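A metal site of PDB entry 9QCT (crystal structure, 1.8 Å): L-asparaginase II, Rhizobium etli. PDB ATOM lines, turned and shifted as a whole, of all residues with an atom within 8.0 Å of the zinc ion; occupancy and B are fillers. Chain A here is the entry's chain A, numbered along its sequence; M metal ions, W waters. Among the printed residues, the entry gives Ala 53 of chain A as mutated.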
ATOM      1  N   ALA A  53      11.661  24.970  20.133  1.00  0.00           N
ATOM      2  CA  ALA A  53      10.741  25.953  19.541  1.00  0.00           C
ATOM      3  C   ALA A  53       9.629  25.176  18.846  1.00  0.00           C
ATOM      4  O   ALA A  53       9.134  24.205  19.427  1.00  0.00           O
ATOM      5  CB  ALA A  53      11.550  26.892  18.639  1.00  0.00           C
ATOM      6  N   SER A  54       9.261  25.513  17.597  1.00  0.00           N
ATOM      7  CA  SER A  54       8.094  24.886  16.975  1.00  0.00           C
ATOM      8  C   SER A  54       8.252  23.398  16.714  1.00  0.00           C
ATOM      9  O   SER A  54       7.229  22.712  16.486  1.00  0.00           O
ATOM     10  CB  SER A  54       7.748  25.564  15.653  1.00  0.00           C
ATOM     11  OG  SER A  54       7.103  26.779  15.947  1.00  0.00           O
ATOM     12  N   LYS A  57       6.112  21.079  18.783  1.00  0.00           N
ATOM     13  CA  LYS A  57       4.660  21.138  18.726  1.00  0.00           C
ATOM     14  C   LYS A  57       3.959  19.770  18.726  1.00  0.00           C
ATOM     15  O   LYS A  57       2.864  19.678  19.325  1.00  0.00           O
ATOM     16  CB  LYS A  57       4.205  21.975  17.515  1.00  0.00           C
ATOM     17  CG  LYS A  57       4.364  23.479  17.823  1.00  0.00           C
ATOM     18  CD  LYS A  57       4.069  24.289  16.573  1.00  0.00           C
ATOM     19  CE  LYS A  57       4.029  25.773  16.917  1.00  0.00           C
ATOM     20  NZ  LYS A  57       4.238  26.605  15.662  1.00  0.00           N
ATOM     21  N   GLN A  60       3.519  19.123  22.279  1.00  0.00           N
ATOM     22  CA  GLN A  60       2.475  19.956  22.861  1.00  0.00           C
ATOM     23  C   GLN A  60       1.099  19.476  22.447  1.00  0.00           C
ATOM     24  O   GLN A  60       0.158  19.510  23.248  1.00  0.00           O
ATOM     25  CB  GLN A  60       2.702  21.421  22.476  1.00  0.00           C
ATOM     26  CG  GLN A  60       3.888  21.992  23.236  1.00  0.00           C
ATOM     27  CD  GLN A  60       4.475  23.173  22.550  1.00  0.00           C
ATOM     28  OE1 GLN A  60       4.812  23.107  21.366  1.00  0.00           O
ATOM     29  NE2 GLN A  60       4.620  24.273  23.289  1.00  0.00           N
ATOM     30  N   MET A  83      -2.721  22.228  15.017  1.00  0.00           N
ATOM     31  CA  MET A  83      -2.090  22.314  16.332  1.00  0.00           C
ATOM     32  C   MET A  83      -0.602  22.050  16.222  1.00  0.00           C
ATOM     33  O   MET A  83       0.192  22.624  16.973  1.00  0.00           O
ATOM     34  CB  MET A  83      -2.734  21.333  17.332  1.00  0.00           C
ATOM     35  CG  MET A  83      -4.174  21.572  17.582  1.00  0.00           C
ATOM     36  SD  MET A  83      -4.709  20.299  18.796  1.00  0.00           S
ATOM     37  CE  MET A  83      -6.515  20.481  18.650  1.00  0.00           C
ATOM     38  N   ALA A  85       1.347  22.954  13.743  1.00  0.00           N
ATOM     39  CA  ALA A  85       1.769  23.762  12.611  1.00  0.00           C
ATOM     40  C   ALA A  85       2.676  24.929  13.000  1.00  0.00           C
ATOM     41  O   ALA A  85       2.579  25.465  14.111  1.00  0.00           O
ATOM     42  CB  ALA A  85       0.541  24.352  11.904  1.00  0.00           C
ATOM     43  N   SER A  86       3.501  25.375  12.034  1.00  0.00           N
ATOM     44  CA  SER A  86       4.029  26.758  11.921  1.00  0.00           C
ATOM     45  C   SER A  86       3.519  27.293  10.583  1.00  0.00           C
ATOM     46  O   SER A  86       4.244  27.355   9.575  1.00  0.00           O
ATOM     47  CB  SER A  86       5.609  26.859  11.986  1.00  0.00           C
ATOM     48  OG  SER A  86       6.110  26.357  13.215  1.00  0.00           O
ATOM     49  N   CYS A 113      -1.454  34.651  22.117  1.00  0.00           N
ATOM     50  CA  CYS A 113      -0.414  34.816  21.114  1.00  0.00           C
ATOM     51  C   CYS A 113      -0.706  36.078  20.312  1.00  0.00           C
ATOM     52  O   CYS A 113      -1.833  36.564  20.262  1.00  0.00           O
ATOM     53  CB  CYS A 113      -0.357  33.594  20.184  1.00  0.00           C
ATOM     54  SG  CYS A 113      -1.971  33.137  19.456  1.00  0.00           S
ATOM     55  N   SER A 139      -1.415  34.167  14.042  1.00  0.00           N
ATOM     56  CA  SER A 139      -0.142  33.593  14.523  1.00  0.00           C
ATOM     57  C   SER A 139       0.123  32.240  13.889  1.00  0.00           C
ATOM     58  O   SER A 139      -0.788  31.392  13.821  1.00  0.00           O
ATOM     59  CB  SER A 139      -0.202  33.443  16.045  1.00  0.00           C
ATOM     60  OG  SER A 139       0.831  32.602  16.538  1.00  0.00           O
ATOM     61  N   ASN A 140       1.389  31.987  13.497  1.00  0.00           N
ATOM     62  CA  ASN A 140       1.758  30.659  13.004  1.00  0.00           C
ATOM     63  C   ASN A 140       1.472  29.576  14.037  1.00  0.00           C
ATOM     64  O   ASN A 140       1.329  28.399  13.677  1.00  0.00           O
ATOM     65  CB  ASN A 140       3.250  30.615  12.586  1.00  0.00           C
ATOM     66  CG  ASN A 140       4.173  30.465  13.776  1.00  0.00           C
ATOM     67  OD1 ASN A 140       4.641  29.372  14.069  1.00  0.00           O
ATOM     68  ND2 ASN A 140       4.375  31.549  14.511  1.00  0.00           N
ATOM     69  N   CYS A 141       1.400  29.955  15.331  1.00  0.00           N
ATOM     70  CA  CYS A 141       1.093  29.070  16.450  1.00  0.00           C
ATOM     71  C   CYS A 141      -0.385  29.003  16.817  1.00  0.00           C
ATOM     72  O   CYS A 141      -0.723  28.470  17.880  1.00  0.00           O
ATOM     73  CB  CYS A 141       1.912  29.509  17.664  1.00  0.00           C
ATOM     74  SG  CYS A 141       3.702  29.339  17.317  1.00  0.00           S
ATOM     75  N   SER A 142      -1.289  29.587  16.006  1.00  0.00           N
ATOM     76  CA  SER A 142      -2.659  29.790  16.463  1.00  0.00           C
ATOM     77  C   SER A 142      -3.350  28.485  16.790  1.00  0.00           C
ATOM     78  O   SER A 142      -4.150  28.426  17.727  1.00  0.00           O
ATOM     79  CB  SER A 142      -3.512  30.552  15.450  1.00  0.00           C
ATOM     80  OG  SER A 142      -3.515  29.877  14.187  1.00  0.00           O
ATOM     81  N   LYS A 144      -2.011  25.623  17.928  1.00  0.00           N
ATOM     82  CA  LYS A 144      -1.540  25.201  19.248  1.00  0.00           C
ATOM     83  C   LYS A 144      -2.248  25.995  20.342  1.00  0.00           C
ATOM     84  O   LYS A 144      -2.708  25.419  21.347  1.00  0.00           O
ATOM     85  CB  LYS A 144      -0.021  25.360  19.344  1.00  0.00           C
ATOM     86  CG  LYS A 144       0.562  25.193  20.756  1.00  0.00           C
ATOM     87  CD  LYS A 144       2.104  25.429  20.802  1.00  0.00           C
ATOM     88  CE  LYS A 144       2.554  26.720  20.061  1.00  0.00           C
ATOM     89  NZ  LYS A 144       3.987  27.012  20.361  1.00  0.00           N
ATOM     90  N   HIS A 145      -2.329  27.325  20.182  1.00  0.00           N
ATOM     91  CA  HIS A 145      -2.996  28.123  21.207  1.00  0.00           C
ATOM     92  C   HIS A 145      -4.468  27.739  21.366  1.00  0.00           C
ATOM     93  O   HIS A 145      -4.976  27.652  22.487  1.00  0.00           O
ATOM     94  CB  HIS A 145      -2.806  29.613  20.913  1.00  0.00           C
ATOM     95  CG  HIS A 145      -1.480  30.111  21.368  1.00  0.00           C
ATOM     96  ND1 HIS A 145      -1.318  30.849  22.527  1.00  0.00           N
ATOM     97  CD2 HIS A 145      -0.229  29.932  20.849  1.00  0.00           C
ATOM     98  CE1 HIS A 145      -0.034  31.126  22.685  1.00  0.00           C
ATOM     99  NE2 HIS A 145       0.645  30.576  21.691  1.00  0.00           N
ATOM    100  N   ASP A 193       8.479  31.681  24.317  1.00  0.00           N
ATOM    101  CA  ASP A 193       8.466  31.609  22.853  1.00  0.00           C
ATOM    102  C   ASP A 193       7.974  32.936  22.249  1.00  0.00           C
ATOM    103  O   ASP A 193       7.445  33.821  22.954  1.00  0.00           O
ATOM    104  CB  ASP A 193       7.566  30.447  22.411  1.00  0.00           C
ATOM    105  CG  ASP A 193       8.118  29.684  21.190  1.00  0.00           C
ATOM    106  OD1 ASP A 193       8.965  30.259  20.460  1.00  0.00           O
ATOM    107  OD2 ASP A 193       7.714  28.510  20.977  1.00  0.00           O
ATOM    108  N   GLY A 194       8.142  33.057  20.918  1.00  0.00           N
ATOM    109  CA  GLY A 194       7.582  34.197  20.215  1.00  0.00           C
ATOM    110  C   GLY A 194       6.075  34.300  20.328  1.00  0.00           C
ATOM    111  O   GLY A 194       5.514  35.401  20.325  1.00  0.00           O
ATOM    112  N   CYS A 195       5.388  33.153  20.443  1.00  0.00           N
ATOM    113  CA  CYS A 195       3.937  33.086  20.599  1.00  0.00           C
ATOM    114  C   CYS A 195       3.470  33.205  22.050  1.00  0.00           C
ATOM    115  O   CYS A 195       2.270  33.098  22.314  1.00  0.00           O
ATOM    116  CB  CYS A 195       3.432  31.768  19.998  1.00  0.00           C
ATOM    117  SG  CYS A 195       3.992  30.376  20.992  1.00  0.00           S
ATOM    118  N   ASN A 196       4.393  33.458  22.994  1.00  0.00           N
ATOM    119  CA  ASN A 196       4.096  33.773  24.393  1.00  0.00           C
ATOM    120  C   ASN A 196       3.753  32.536  25.229  1.00  0.00           C
ATOM    121  O   ASN A 196       3.151  32.674  26.295  1.00  0.00           O
ATOM    122  CB  ASN A 196       2.994  34.814  24.513  1.00  0.00           C
ATOM    123  CG  ASN A 196       3.127  35.662  25.772  1.00  0.00           C
ATOM    124  OD1 ASN A 196       4.247  35.881  26.279  1.00  0.00           O
ATOM    125  ND2 ASN A 196       1.988  36.172  26.276  1.00  0.00           N
ATOM    126  N   LEU A 197       4.131  31.338  24.810  1.00  0.00           N
ATOM    127  CA  LEU A 197       4.041  30.101  25.584  1.00  0.00           C
ATOM    128  C   LEU A 197       5.410  29.690  26.088  1.00  0.00           C
ATOM    129  O   LEU A 197       6.446  30.049  25.484  1.00  0.00           O
ATOM    130  CB  LEU A 197       3.475  28.958  24.724  1.00  0.00           C
ATOM    131  CG  LEU A 197       1.941  28.914  24.521  1.00  0.00           C
ATOM    132  CD1 LEU A 197       1.603  27.866  23.444  1.00  0.00           C
ATOM    133  CD2 LEU A 197       1.241  28.583  25.845  1.00  0.00           C
ATOM    134  N   PRO A 198       5.478  28.898  27.165  1.00  0.00           N
ATOM    135  CA  PRO A 198       6.754  28.272  27.539  1.00  0.00           C
ATOM    136  C   PRO A 198       7.259  27.420  26.380  1.00  0.00           C
ATOM    137  O   PRO A 198       6.484  26.784  25.666  1.00  0.00           O
ATOM    138  CB  PRO A 198       6.390  27.419  28.773  1.00  0.00           C
ATOM    139  CG  PRO A 198       5.122  28.030  29.316  1.00  0.00           C
ATOM    140  CD  PRO A 198       4.383  28.464  28.050  1.00  0.00           C
ATOM    141  N   THR A 199       8.578  27.484  26.157  1.00  0.00           N
ATOM    142  CA  THR A 199       9.167  26.649  25.118  1.00  0.00           C
ATOM    143  C   THR A 199      10.372  25.903  25.679  1.00  0.00           C
ATOM    144  O   THR A 199      11.136  26.476  26.460  1.00  0.00           O
ATOM    145  CB  THR A 199       9.555  27.470  23.877  1.00  0.00           C
ATOM    146  OG1 THR A 199      10.062  26.590  22.867  1.00  0.00           O
ATOM    147  CG2 THR A 199      10.598  28.582  24.194  1.00  0.00           C
HETATM  148 ZN    ZN M   1       4.496  28.805  19.418  1.00  0.00          ZN
HETATM  149  O   HOH W   1       6.460  28.395  18.785  1.00  0.00           O
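The zinc ion is bound by NZ of Lys 144 (2.1 Å), water W1 (2.1 Å), SG of Cys 195 (2.3 Å) and SG of Cys 141 (2.3 Å). The zinc ion has four donor atoms within binding distance.
The backbone carbonyl oxygen of Cys 195 sits close to a ring nitrogen (NE2) of His 145 (3.1 Å). SG of Cys 141 lies close to NZ of Lys 57, 3.2 Å away. SG of Cys 141 lies close to OD1 of Asn 140 (3.4 Å). N of Cys 141 is in hydrogen-bond range of OG of Ser 139, at 3.0 Å. The side-chain amino group (NZ) of Lys 57 sits at hydrogen-bond distance from the side-chain hydroxyl (OG) of Ser 54 (2.9 Å). OD1 of Asn 140 sits at hydrogen-bond distance from NZ of Lys 57 (3.2 Å). NZ of Lys 57 is in hydrogen-bond range of O of Ala 85 (2.5 Å). NZ of Lys 57 is in hydrogen-bond range of OG of Ser 86, at 3.1 Å.
Merely in contact with the zinc ion: Lys 57 and Asp 193. Of the 21 residues printed, 5 come within 4 Å of the zinc ion.
Water W1 bridges the side-chain carboxylate (OD2) of Asp 193 and the side-chain hydroxyl (OG) of Ser 54.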
